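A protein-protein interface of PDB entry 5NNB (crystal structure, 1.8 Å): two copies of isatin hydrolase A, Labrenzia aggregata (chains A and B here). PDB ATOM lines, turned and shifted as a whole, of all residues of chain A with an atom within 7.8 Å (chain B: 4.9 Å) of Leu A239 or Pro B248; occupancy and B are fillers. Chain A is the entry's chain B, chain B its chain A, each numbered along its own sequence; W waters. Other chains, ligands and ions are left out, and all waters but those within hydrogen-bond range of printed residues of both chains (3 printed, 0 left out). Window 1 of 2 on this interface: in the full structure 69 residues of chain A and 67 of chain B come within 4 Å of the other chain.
Of the 25 printed residues of chain A, 13 touch a printed residue of chain B.
Hydrophobic or aromatic side chains of chain A that line the printed part of chain B: His A62, Ile A64, Phe A99, Ala A237 and Leu A239.
Among the printed residues, 18 pairs touch across the chains.
Pro A238 touches Arg B250, and with the chains exchanged Arg A250 touches Pro B238.
Leu A239 touches Pro B248, and with the chains exchanged Pro A248 touches Leu B239.
Leu A239 touches Leu B249, and with the chains exchanged Leu A249 touches Leu B239.
Arg A250 touches Leu B239, but with the chains exchanged Leu A239 does not touch Arg B250 (4.02 Å).
10 positions are printed for both chains.
Of the 18 pairs that touch across the chains among the printed residues, 6 have their exchanged pair printed and touching as well.
N of Ser B67 sits at hydrogen-bond distance from OG1 of Thr B70 (2.8 Å).
N of Ser B247 lies close to O of Glu B68.
The backbone carbonyl oxygen (O) of Thr B72 sits at hydrogen-bond distance from the backbone NH (N) of Leu B249, at 3.2 Å.
N of Val A91 is in hydrogen-bond range of O of Gly A244 (2.9 Å).
The backbone carbonyl oxygen of Phe A99 is in hydrogen-bond range of the backbone NH of Ala A236 (2.8 Å).
OG of Ser A247 is in hydrogen-bond range of N of Leu A239, 2.9 Å away.
His A62 touches Ser B67 (O to CA, 3.4 Å).
Phe A99 touches Arg B250.
O of Ala A237 touches CB of Arg B250 (3.6 Å).
CB of Leu A239 touches CD1 of Leu B25 (3.9 Å).
CD2 of Leu A239 touches O of Pro B248, at 3.6 Å.
CZ of Arg B250 touches CG of Lys A240, 3.6 Å away.
O of Leu B25 touches CA of Ile A241, 3.9 Å away.
CD2 of Leu B239 touches O of Pro A248 (3.6 Å).
Leu A249 touches Leu B239.
NH1 of Arg A250 touches O of Leu B239, at 3.9 Å.
O of Lys A240 sits at hydrogen-bond distance from N of Leu B25.
The backbone carbonyl oxygen (O) of Leu B25 is in hydrogen-bond range of the backbone NH (N) of Lys A242 (3.0 Å).
The backbone carbonyl oxygen (O) of Met B66 lies within hydrogen-bond range of the backbone NH (N) of Ile A64.
The side-chain carboxylate (OE1) of Glu B68 is in hydrogen-bond range of the backbone NH (N) of His A62 (2.7 Å).
The guanidinium group of Arg A250 is in hydrogen-bond range of the backbone carbonyl oxygen of Pro B238 (3.0 Å).
The guanidinium group (NH1) of Arg B250 lies within hydrogen-bond range of the backbone carbonyl oxygen (O) of Val A91 (3.3 Å).
O of Pro A238 sits at hydrogen-bond distance from NH1 of Arg B250, at 3.0 Å.
Printed residues of chain B within 4 Å of Leu A239: Leu B25, Pro B248 and Leu B249.
Pro B248 touches one residue of chain A.
No residue of chain A comes within 4 Å of Ser B247.
Printed residues of chain B within 4 Å of Leu A249: Leu B239 (3.6 Å).
Printed residues of chain B within 4 Å of Ile A64: Met B66 (2.7 Å).
Printed residues of chain B within 4 Å of His A62: Ser B67 and Glu B68.
Of the printed residues of chain A, Met B66 touches Ile A64 (2.7 Å).
Ser A90 touches none of the printed residues of chain B.
The nearest printed residue of chain B that does not touch Leu A239 is Arg B250 (4.02 Å).
The nearest printed residue of chain A that does not touch Met B66 is Met A66 (4.2 Å).
Water W3 bridges O of Ala A237 and N of Arg B250.
Water W1 lies within hydrogen-bond range of O of Val A91, NH2 of Arg B250, O of Asp A92 and N of Glu A93.
Water W2 bridges the backbone NH (N) of Lys A240 (2.9 Å) and the backbone carbonyl oxygen (O) of Leu B249 (3.1 Å).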
ATOM      1  N   HIS A  62      23.209  20.960 -22.956  1.00  0.00           N
ATOM      2  CA  HIS A  62      24.434  20.178 -23.114  1.00  0.00           C
ATOM      3  C   HIS A  62      24.194  18.680 -23.282  1.00  0.00           C
ATOM      4  O   HIS A  62      23.193  18.130 -22.795  1.00  0.00           O
ATOM      5  CB  HIS A  62      25.351  20.349 -21.886  1.00  0.00           C
ATOM      6  CG  HIS A  62      25.722  21.760 -21.578  1.00  0.00           C
ATOM      7  ND1 HIS A  62      24.975  22.563 -20.747  1.00  0.00           N
ATOM      8  CD2 HIS A  62      26.805  22.497 -21.940  1.00  0.00           C
ATOM      9  CE1 HIS A  62      25.550  23.747 -20.644  1.00  0.00           C
ATOM     10  NE2 HIS A  62      26.669  23.728 -21.352  1.00  0.00           N
ATOM     11  N   ILE A  64      26.032  15.210 -21.986  1.00  0.00           N
ATOM     12  CA  ILE A  64      26.909  14.879 -20.870  1.00  0.00           C
ATOM     13  C   ILE A  64      27.317  13.405 -20.950  1.00  0.00           C
ATOM     14  O   ILE A  64      26.582  12.571 -21.478  1.00  0.00           O
ATOM     15  CB  ILE A  64      26.243  15.184 -19.498  1.00  0.00           C
ATOM     16  CG1 ILE A  64      24.926  14.409 -19.339  1.00  0.00           C
ATOM     17  CG2 ILE A  64      25.968  16.661 -19.357  1.00  0.00           C
ATOM     18  CD1 ILE A  64      24.159  14.751 -18.077  1.00  0.00           C
ATOM     19  N   MET A  66      29.622  10.343 -18.515  1.00  0.00           N
ATOM     20  CA  MET A  66      30.239  10.001 -17.238  1.00  0.00           C
ATOM     21  C   MET A  66      30.133   8.493 -17.077  1.00  0.00           C
ATOM     22  O   MET A  66      29.743   7.785 -18.013  1.00  0.00           O
ATOM     23  CB  MET A  66      29.547  10.733 -16.084  1.00  0.00           C
ATOM     24  CG  MET A  66      28.135  10.230 -15.793  1.00  0.00           C
ATOM     25  SD  MET A  66      26.933  11.542 -15.615  1.00  0.00           S
ATOM     26  CE  MET A  66      26.899  12.153 -17.299  1.00  0.00           C
ATOM     27  N   SER A  67      30.484   7.989 -15.902  1.00  0.00           N
ATOM     28  CA  SER A  67      30.178   6.608 -15.588  1.00  0.00           C
ATOM     29  C   SER A  67      29.093   6.582 -14.520  1.00  0.00           C
ATOM     30  O   SER A  67      28.778   7.611 -13.914  1.00  0.00           O
ATOM     31  CB  SER A  67      31.436   5.847 -15.153  1.00  0.00           C
ATOM     32  OG  SER A  67      31.727   6.058 -13.787  1.00  0.00           O
ATOM     33  N   GLU A  68      28.505   5.414 -14.292  1.00  0.00           N
ATOM     34  CA  GLU A  68      27.556   5.265 -13.200  1.00  0.00           C
ATOM     35  C   GLU A  68      28.139   5.662 -11.849  1.00  0.00           C
ATOM     36  O   GLU A  68      27.397   6.078 -10.955  1.00  0.00           O
ATOM     37  CB  GLU A  68      27.060   3.822 -13.120  1.00  0.00           C
ATOM     38  CG  GLU A  68      26.237   3.369 -14.300  1.00  0.00           C
ATOM     39  CD  GLU A  68      25.980   1.885 -14.258  1.00  0.00           C
ATOM     40  OE1 GLU A  68      26.911   1.135 -13.909  1.00  0.00           O
ATOM     41  OE2 GLU A  68      24.852   1.464 -14.565  1.00  0.00           O
ATOM     42  N   PHE A  74      25.514   6.785  -6.044  1.00  0.00           N
ATOM     43  CA  PHE A  74      24.792   5.723  -5.334  1.00  0.00           C
ATOM     44  C   PHE A  74      25.255   4.387  -5.914  1.00  0.00           C
ATOM     45  O   PHE A  74      25.380   4.251  -7.124  1.00  0.00           O
ATOM     46  CB  PHE A  74      23.258   5.947  -5.526  1.00  0.00           C
ATOM     47  CG  PHE A  74      22.349   4.919  -4.860  1.00  0.00           C
ATOM     48  CD1 PHE A  74      22.248   3.623  -5.352  1.00  0.00           C
ATOM     49  CD2 PHE A  74      21.485   5.309  -3.841  1.00  0.00           C
ATOM     50  CE1 PHE A  74      21.366   2.700  -4.784  1.00  0.00           C
ATOM     51  CE2 PHE A  74      20.596   4.403  -3.261  1.00  0.00           C
ATOM     52  CZ  PHE A  74      20.535   3.093  -3.736  1.00  0.00           C
ATOM     53  N   SER A  90      19.471  -3.757  -9.283  1.00  0.00           N
ATOM     54  CA  SER A  90      19.875  -2.593 -10.091  1.00  0.00           C
ATOM     55  C   SER A  90      19.099  -1.312  -9.704  1.00  0.00           C
ATOM     56  O   SER A  90      18.018  -1.400  -9.126  1.00  0.00           O
ATOM     57  CB  SER A  90      19.694  -2.908 -11.580  1.00  0.00           C
ATOM     58  OG  SER A  90      18.363  -3.320 -11.875  1.00  0.00           O
ATOM     59  N   VAL A  91      19.625  -0.121 -10.030  1.00  0.00           N
ATOM     60  CA  VAL A  91      19.007   1.125  -9.544  1.00  0.00           C
ATOM     61  C   VAL A  91      17.561   1.333 -10.011  1.00  0.00           C
ATOM     62  O   VAL A  91      16.803   2.067  -9.381  1.00  0.00           O
ATOM     63  CB  VAL A  91      19.792   2.401  -9.973  1.00  0.00           C
ATOM     64  CG1 VAL A  91      21.032   2.554  -9.135  1.00  0.00           C
ATOM     65  CG2 VAL A  91      20.121   2.382 -11.479  1.00  0.00           C
ATOM     66  N   ASP A  92      17.187   0.713 -11.120  1.00  0.00           N
ATOM     67  CA  ASP A  92      15.833   0.895 -11.641  1.00  0.00           C
ATOM     68  C   ASP A  92      14.841  -0.038 -10.963  1.00  0.00           C
ATOM     69  O   ASP A  92      13.628   0.090 -11.156  1.00  0.00           O
ATOM     70  CB  ASP A  92      15.801   0.652 -13.146  1.00  0.00           C
ATOM     71  CG  ASP A  92      16.242  -0.759 -13.527  1.00  0.00           C
ATOM     72  OD1 ASP A  92      17.125  -1.333 -12.862  1.00  0.00           O
ATOM     73  OD2 ASP A  92      15.703  -1.297 -14.508  1.00  0.00           O
ATOM     74  N   GLU A  93      15.354  -0.956 -10.148  1.00  0.00           N
ATOM     75  CA  GLU A  93      14.499  -1.976  -9.522  1.00  0.00           C
ATOM     76  C   GLU A  93      14.318  -1.795  -8.006  1.00  0.00           C
ATOM     77  O   GLU A  93      13.407  -2.372  -7.396  1.00  0.00           O
ATOM     78  CB  GLU A  93      15.072  -3.356  -9.793  1.00  0.00           C
ATOM     79  CG  GLU A  93      15.135  -3.751 -11.248  1.00  0.00           C
ATOM     80  CD  GLU A  93      15.909  -5.040 -11.447  1.00  0.00           C
ATOM     81  OE1 GLU A  93      15.895  -5.579 -12.577  1.00  0.00           O
ATOM     82  OE2 GLU A  93      16.535  -5.511 -10.465  1.00  0.00           O
ATOM     83  N   PHE A  99      14.559   5.433  -0.902  1.00  0.00           N
ATOM     84  CA  PHE A  99      15.245   6.655  -1.352  1.00  0.00           C
ATOM     85  C   PHE A  99      15.069   7.822  -0.388  1.00  0.00           C
ATOM     86  O   PHE A  99      15.742   8.839  -0.495  1.00  0.00           O
ATOM     87  CB  PHE A  99      14.721   7.056  -2.741  1.00  0.00           C
ATOM     88  CG  PHE A  99      14.972   6.024  -3.803  1.00  0.00           C
ATOM     89  CD1 PHE A  99      16.030   5.137  -3.683  1.00  0.00           C
ATOM     90  CD2 PHE A  99      14.155   5.937  -4.923  1.00  0.00           C
ATOM     91  CE1 PHE A  99      16.262   4.185  -4.658  1.00  0.00           C
ATOM     92  CE2 PHE A  99      14.395   4.986  -5.905  1.00  0.00           C
ATOM     93  CZ  PHE A  99      15.449   4.113  -5.766  1.00  0.00           C
ATOM     94  N   ALA A 236      18.036  10.256  -1.164  1.00  0.00           N
ATOM     95  CA  ALA A 236      19.033   9.718  -2.084  1.00  0.00           C
ATOM     96  C   ALA A 236      18.355   8.844  -3.129  1.00  0.00           C
ATOM     97  O   ALA A 236      18.302   7.607  -2.987  1.00  0.00           O
ATOM     98  CB  ALA A 236      20.122   8.919  -1.319  1.00  0.00           C
ATOM     99  N   ALA A 237      17.831   9.496  -4.173  1.00  0.00           N
ATOM    100  CA  ALA A 237      17.113   8.812  -5.242  1.00  0.00           C
ATOM    101  C   ALA A 237      17.958   8.731  -6.505  1.00  0.00           C
ATOM    102  O   ALA A 237      18.115   9.727  -7.213  1.00  0.00           O
ATOM    103  CB  ALA A 237      15.769   9.540  -5.542  1.00  0.00           C
ATOM    104  N   PRO A 238      18.486   7.538  -6.817  1.00  0.00           N
ATOM    105  CA  PRO A 238      19.342   7.414  -8.002  1.00  0.00           C
ATOM    106  C   PRO A 238      18.556   7.473  -9.304  1.00  0.00           C
ATOM    107  O   PRO A 238      17.346   7.198  -9.306  1.00  0.00           O
ATOM    108  CB  PRO A 238      19.985   6.037  -7.830  1.00  0.00           C
ATOM    109  CG  PRO A 238      18.954   5.260  -7.041  1.00  0.00           C
ATOM    110  CD  PRO A 238      18.342   6.259  -6.102  1.00  0.00           C
ATOM    111  N   LEU A 239      19.252   7.814 -10.389  1.00  0.00           N
ATOM    112  CA  LEU A 239      18.664   7.802 -11.730  1.00  0.00           C
ATOM    113  C   LEU A 239      18.098   6.430 -12.046  1.00  0.00           C
ATOM    114  O   LEU A 239      18.675   5.403 -11.657  1.00  0.00           O
ATOM    115  CB  LEU A 239      19.703   8.176 -12.779  1.00  0.00           C
ATOM    116  CG  LEU A 239      20.320   9.555 -12.580  1.00  0.00           C
ATOM    117  CD1 LEU A 239      21.400   9.815 -13.630  1.00  0.00           C
ATOM    118  CD2 LEU A 239      19.254  10.612 -12.613  1.00  0.00           C
ATOM    119  N   LYS A 240      16.979   6.401 -12.764  1.00  0.00           N
ATOM    120  CA  LYS A 240      16.338   5.125 -13.050  1.00  0.00           C
ATOM    121  C   LYS A 240      16.962   4.463 -14.280  1.00  0.00           C
ATOM    122  O   LYS A 240      16.269   4.169 -15.244  1.00  0.00           O
ATOM    123  CB  LYS A 240      14.832   5.321 -13.247  1.00  0.00           C
ATOM    124  CG  LYS A 240      14.004   4.077 -13.020  1.00  0.00           C
ATOM    125  CD  LYS A 240      12.519   4.394 -13.141  1.00  0.00           C
ATOM    126  CE  LYS A 240      11.687   3.166 -12.822  1.00  0.00           C
ATOM    127  NZ  LYS A 240      10.257   3.537 -12.817  1.00  0.00           N
ATOM    128  N   ILE A 241      18.271   4.198 -14.220  1.00  0.00           N
ATOM    129  CA  ILE A 241      19.005   3.601 -15.332  1.00  0.00           C
ATOM    130  C   ILE A 241      18.648   2.125 -15.513  1.00  0.00           C
ATOM    131  O   ILE A 241      18.726   1.348 -14.557  1.00  0.00           O
ATOM    132  CB  ILE A 241      20.543   3.723 -15.125  1.00  0.00           C
ATOM    133  CG1 ILE A 241      20.964   5.194 -15.088  1.00  0.00           C
ATOM    134  CG2 ILE A 241      21.273   2.975 -16.226  1.00  0.00           C
ATOM    135  CD1 ILE A 241      22.479   5.418 -14.765  1.00  0.00           C
ATOM    136  N   LYS A 242      18.238   1.745 -16.727  1.00  0.00           N
ATOM    137  CA  LYS A 242      17.886   0.349 -17.011  1.00  0.00           C
ATOM    138  C   LYS A 242      19.069  -0.575 -16.694  1.00  0.00           C
ATOM    139  O   LYS A 242      20.160  -0.418 -17.255  1.00  0.00           O
ATOM    140  CB  LYS A 242      17.448   0.173 -18.469  1.00  0.00           C
ATOM    141  CG  LYS A 242      17.051  -1.258 -18.834  1.00  0.00           C
ATOM    142  CD  LYS A 242      15.851  -1.726 -17.983  1.00  0.00           C
ATOM    143  CE  LYS A 242      15.402  -3.150 -18.303  1.00  0.00           C
ATOM    144  NZ  LYS A 242      16.083  -4.183 -17.449  1.00  0.00           N
ATOM    145  N   GLY A 244      20.984  -0.509 -14.259  1.00  0.00           N
ATOM    146  CA  GLY A 244      22.121   0.259 -13.783  1.00  0.00           C
ATOM    147  C   GLY A 244      22.699  -0.261 -12.475  1.00  0.00           C
ATOM    148  O   GLY A 244      21.952  -0.681 -11.592  1.00  0.00           O
ATOM    149  N   THR A 245      24.026  -0.199 -12.332  1.00  0.00           N
ATOM    150  CA  THR A 245      24.676  -0.686 -11.111  1.00  0.00           C
ATOM    151  C   THR A 245      24.810   0.453 -10.110  1.00  0.00           C
ATOM    152  O   THR A 245      25.313   0.282  -9.005  1.00  0.00           O
ATOM    153  CB  THR A 245      26.090  -1.273 -11.389  1.00  0.00           C
ATOM    154  OG1 THR A 245      27.006  -0.212 -11.669  1.00  0.00           O
ATOM    155  CG2 THR A 245      26.075  -2.245 -12.568  1.00  0.00           C
ATOM    156  N   GLY A 246      24.380   1.637 -10.519  1.00  0.00           N
ATOM    157  CA  GLY A 246      24.466   2.804  -9.675  1.00  0.00           C
ATOM    158  C   GLY A 246      24.275   4.034 -10.542  1.00  0.00           C
ATOM    159  O   GLY A 246      23.991   3.908 -11.736  1.00  0.00           O
ATOM    160  N   SER A 247      24.391   5.213  -9.944  1.00  0.00           N
ATOM    161  CA  SER A 247      24.341   6.469 -10.724  1.00  0.00           C
ATOM    162  C   SER A 247      24.731   7.672  -9.896  1.00  0.00           C
ATOM    163  O   SER A 247      24.558   7.681  -8.678  1.00  0.00           O
ATOM    164  CB  SER A 247      22.933   6.705 -11.302  1.00  0.00           C
ATOM    165  OG  SER A 247      22.118   7.399 -10.367  1.00  0.00           O
ATOM    166  N   PRO A 248      25.242   8.720 -10.556  1.00  0.00           N
ATOM    167  CA  PRO A 248      25.341   9.995  -9.853  1.00  0.00           C
ATOM    168  C   PRO A 248      23.957  10.446  -9.418  1.00  0.00           C
ATOM    169  O   PRO A 248      22.960  10.085 -10.055  1.00  0.00           O
ATOM    170  CB  PRO A 248      25.933  10.946 -10.909  1.00  0.00           C
ATOM    171  CG  PRO A 248      26.585  10.068 -11.902  1.00  0.00           C
ATOM    172  CD  PRO A 248      25.748   8.801 -11.931  1.00  0.00           C
ATOM    173  N   LEU A 249      23.872  11.223  -8.345  1.00  0.00           N
ATOM    174  CA  LEU A 249      22.565  11.695  -7.905  1.00  0.00           C
ATOM    175  C   LEU A 249      22.755  12.917  -7.050  1.00  0.00           C
ATOM    176  O   LEU A 249      23.867  13.206  -6.613  1.00  0.00           O
ATOM    177  CB  LEU A 249      21.801  10.606  -7.124  1.00  0.00           C
ATOM    178  CG  LEU A 249      22.178  10.352  -5.663  1.00  0.00           C
ATOM    179  CD1 LEU A 249      21.253   9.279  -5.047  1.00  0.00           C
ATOM    180  CD2 LEU A 249      23.626   9.913  -5.535  1.00  0.00           C
ATOM    181  N   ARG A 250      21.665  13.645  -6.847  1.00  0.00           N
ATOM    182  CA  ARG A 250      21.649  14.767  -5.922  1.00  0.00           C
ATOM    183  C   ARG A 250      21.215  14.279  -4.533  1.00  0.00           C
ATOM    184  O   ARG A 250      20.044  13.972  -4.296  1.00  0.00           O
ATOM    185  CB  ARG A 250      20.714  15.868  -6.434  1.00  0.00           C
ATOM    186  CG  ARG A 250      20.915  17.217  -5.777  1.00  0.00           C
ATOM    187  CD  ARG A 250      22.223  17.805  -6.241  1.00  0.00           C
ATOM    188  NE  ARG A 250      22.453  19.161  -5.777  1.00  0.00           N
ATOM    189  CZ  ARG A 250      22.184  20.258  -6.486  1.00  0.00           C
ATOM    190  NH1 ARG A 250      21.604  20.172  -7.683  1.00  0.00           N
ATOM    191  NH2 ARG A 250      22.469  21.450  -5.979  1.00  0.00           N
ATOM    192  N   LEU B  25      15.438   5.259 -17.683  1.00  0.00           N
ATOM    193  CA  LEU B  25      16.437   5.770 -18.626  1.00  0.00           C
ATOM    194  C   LEU B  25      16.960   4.623 -19.473  1.00  0.00           C
ATOM    195  O   LEU B  25      17.558   3.675 -18.954  1.00  0.00           O
ATOM    196  CB  LEU B  25      17.597   6.457 -17.903  1.00  0.00           C
ATOM    197  CG  LEU B  25      17.354   7.889 -17.454  1.00  0.00           C
ATOM    198  CD1 LEU B  25      18.395   8.315 -16.440  1.00  0.00           C
ATOM    199  CD2 LEU B  25      17.372   8.826 -18.681  1.00  0.00           C
ATOM    200  N   MET B  66      24.147  11.072 -22.220  1.00  0.00           N
ATOM    201  CA  MET B  66      22.789  11.549 -22.470  1.00  0.00           C
ATOM    202  C   MET B  66      22.821  13.052 -22.663  1.00  0.00           C
ATOM    203  O   MET B  66      23.894  13.662 -22.731  1.00  0.00           O
ATOM    204  CB  MET B  66      21.869  11.182 -21.295  1.00  0.00           C
ATOM    205  CG  MET B  66      22.182  11.946 -19.994  1.00  0.00           C
ATOM    206  SD  MET B  66      22.221  10.950 -18.481  1.00  0.00           S
ATOM    207  CE  MET B  66      23.653   9.933 -18.826  1.00  0.00           C
ATOM    208  N   SER B  67      21.650  13.669 -22.724  1.00  0.00           N
ATOM    209  CA  SER B  67      21.594  15.115 -22.663  1.00  0.00           C
ATOM    210  C   SER B  67      21.080  15.499 -21.309  1.00  0.00           C
ATOM    211  O   SER B  67      20.543  14.660 -20.571  1.00  0.00           O
ATOM    212  CB  SER B  67      20.679  15.693 -23.756  1.00  0.00           C
ATOM    213  OG  SER B  67      21.176  15.374 -25.039  1.00  0.00           O
ATOM    214  N   GLU B  68      21.256  16.761 -20.965  1.00  0.00           N
ATOM    215  CA  GLU B  68      20.625  17.328 -19.794  1.00  0.00           C
ATOM    216  C   GLU B  68      19.110  17.179 -19.879  1.00  0.00           C
ATOM    217  O   GLU B  68      18.442  17.115 -18.853  1.00  0.00           O
ATOM    218  CB  GLU B  68      21.000  18.796 -19.649  1.00  0.00           C
ATOM    219  CG  GLU B  68      22.467  19.037 -19.307  1.00  0.00           C
ATOM    220  CD  GLU B  68      22.806  20.503 -19.439  1.00  0.00           C
ATOM    221  OE1 GLU B  68      22.341  21.099 -20.421  1.00  0.00           O
ATOM    222  OE2 GLU B  68      23.472  21.078 -18.558  1.00  0.00           O
ATOM    223  N   THR B  70      17.254  14.687 -21.408  1.00  0.00           N
ATOM    224  CA  THR B  70      16.881  13.328 -21.784  1.00  0.00           C
ATOM    225  C   THR B  70      15.968  12.711 -20.728  1.00  0.00           C
ATOM    226  O   THR B  70      16.264  12.772 -19.535  1.00  0.00           O
ATOM    227  CB  THR B  70      18.149  12.427 -21.952  1.00  0.00           C
ATOM    228  OG1 THR B  70      18.988  12.953 -22.987  1.00  0.00           O
ATOM    229  CG2 THR B  70      17.779  10.999 -22.302  1.00  0.00           C
ATOM    230  N   THR B  72      12.858  11.575 -18.149  1.00  0.00           N
ATOM    231  CA  THR B  72      12.295  12.308 -17.023  1.00  0.00           C
ATOM    232  C   THR B  72      13.358  13.281 -16.546  1.00  0.00           C
ATOM    233  O   THR B  72      14.406  12.867 -16.070  1.00  0.00           O
ATOM    234  CB  THR B  72      11.865  11.356 -15.858  1.00  0.00           C
ATOM    235  OG1 THR B  72      10.960  10.367 -16.359  1.00  0.00           O
ATOM    236  CG2 THR B  72      11.171  12.143 -14.756  1.00  0.00           C
ATOM    237  N   HIS B  73      13.123  14.572 -16.723  1.00  0.00           N
ATOM    238  CA  HIS B  73      14.158  15.535 -16.419  1.00  0.00           C
ATOM    239  C   HIS B  73      13.611  16.888 -15.995  1.00  0.00           C
ATOM    240  O   HIS B  73      12.417  17.203 -16.145  1.00  0.00           O
ATOM    241  CB  HIS B  73      15.116  15.699 -17.614  1.00  0.00           C
ATOM    242  CG  HIS B  73      14.552  16.467 -18.773  1.00  0.00           C
ATOM    243  ND1 HIS B  73      13.803  15.883 -19.773  1.00  0.00           N
ATOM    244  CD2 HIS B  73      14.654  17.782 -19.101  1.00  0.00           C
ATOM    245  CE1 HIS B  73      13.472  16.802 -20.670  1.00  0.00           C
ATOM    246  NE2 HIS B  73      13.979  17.958 -20.283  1.00  0.00           N
ATOM    247  N   PRO B 238      17.666  17.789  -9.123  1.00  0.00           N
ATOM    248  CA  PRO B 238      18.461  17.531 -10.323  1.00  0.00           C
ATOM    249  C   PRO B 238      19.946  17.312  -9.989  1.00  0.00           C
ATOM    250  O   PRO B 238      20.395  17.718  -8.917  1.00  0.00           O
ATOM    251  CB  PRO B 238      18.273  18.813 -11.151  1.00  0.00           C
ATOM    252  CG  PRO B 238      18.101  19.883 -10.107  1.00  0.00           C
ATOM    253  CD  PRO B 238      17.340  19.217  -8.971  1.00  0.00           C
ATOM    254  N   LEU B 239      20.671  16.675 -10.897  1.00  0.00           N
ATOM    255  CA  LEU B 239      22.132  16.528 -10.783  1.00  0.00           C
ATOM    256  C   LEU B 239      22.821  17.893 -10.666  1.00  0.00           C
ATOM    257  O   LEU B 239      22.395  18.869 -11.287  1.00  0.00           O
ATOM    258  CB  LEU B 239      22.670  15.760 -11.986  1.00  0.00           C
ATOM    259  CG  LEU B 239      22.134  14.347 -12.186  1.00  0.00           C
ATOM    260  CD1 LEU B 239      22.674  13.729 -13.455  1.00  0.00           C
ATOM    261  CD2 LEU B 239      22.488  13.497 -10.992  1.00  0.00           C
ATOM    262  N   GLY B 246      19.813  21.784 -16.871  1.00  0.00           N
ATOM    263  CA  GLY B 246      18.837  20.784 -16.442  1.00  0.00           C
ATOM    264  C   GLY B 246      19.535  19.454 -16.221  1.00  0.00           C
ATOM    265  O   GLY B 246      20.760  19.382 -16.282  1.00  0.00           O
ATOM    266  N   SER B 247      18.784  18.397 -15.911  1.00  0.00           N
ATOM    267  CA  SER B 247      19.374  17.077 -15.833  1.00  0.00           C
ATOM    268  C   SER B 247      18.283  16.028 -15.739  1.00  0.00           C
ATOM    269  O   SER B 247      17.184  16.334 -15.283  1.00  0.00           O
ATOM    270  CB  SER B 247      20.301  16.947 -14.628  1.00  0.00           C
ATOM    271  OG  SER B 247      19.579  16.504 -13.497  1.00  0.00           O
ATOM    272  N   PRO B 248      18.577  14.802 -16.197  1.00  0.00           N
ATOM    273  CA  PRO B 248      17.667  13.706 -15.842  1.00  0.00           C
ATOM    274  C   PRO B 248      17.660  13.585 -14.323  1.00  0.00           C
ATOM    275  O   PRO B 248      18.628  14.003 -13.689  1.00  0.00           O
ATOM    276  CB  PRO B 248      18.289  12.487 -16.525  1.00  0.00           C
ATOM    277  CG  PRO B 248      19.167  13.056 -17.614  1.00  0.00           C
ATOM    278  CD  PRO B 248      19.670  14.352 -17.077  1.00  0.00           C
ATOM    279  N   LEU B 249      16.583  13.080 -13.735  1.00  0.00           N
ATOM    280  CA  LEU B 249      16.547  12.924 -12.284  1.00  0.00           C
ATOM    281  C   LEU B 249      15.484  11.920 -11.907  1.00  0.00           C
ATOM    282  O   LEU B 249      14.618  11.592 -12.715  1.00  0.00           O
ATOM    283  CB  LEU B 249      16.282  14.259 -11.564  1.00  0.00           C
ATOM    284  CG  LEU B 249      14.841  14.782 -11.492  1.00  0.00           C
ATOM    285  CD1 LEU B 249      14.769  16.054 -10.667  1.00  0.00           C
ATOM    286  CD2 LEU B 249      14.265  15.016 -12.893  1.00  0.00           C
ATOM    287  N   ARG B 250      15.560  11.445 -10.672  1.00  0.00           N
ATOM    288  CA  ARG B 250      14.516  10.581 -10.118  1.00  0.00           C
ATOM    289  C   ARG B 250      13.467  11.440  -9.401  1.00  0.00           C
ATOM    290  O   ARG B 250      13.689  11.917  -8.295  1.00  0.00           O
ATOM    291  CB  ARG B 250      15.134   9.560  -9.155  1.00  0.00           C
ATOM    292  CG  ARG B 250      14.234   8.365  -8.868  1.00  0.00           C
ATOM    293  CD  ARG B 250      14.170   7.474 -10.100  1.00  0.00           C
ATOM    294  NE  ARG B 250      13.438   6.225  -9.889  1.00  0.00           N
ATOM    295  CZ  ARG B 250      14.013   5.060  -9.600  1.00  0.00           C
ATOM    296  NH1 ARG B 250      15.331   4.983  -9.472  1.00  0.00           N
ATOM    297  NH2 ARG B 250      13.264   3.976  -9.446  1.00  0.00           N
HETATM  298  O   HOH W   1      14.414   1.781  -8.302  1.00  0.00           O
HETATM  299  O   HOH W   2      16.185   9.052 -13.695  1.00  0.00           O
HETATM  300  O   HOH W   3      17.920  11.499  -9.066  1.00  0.00           O
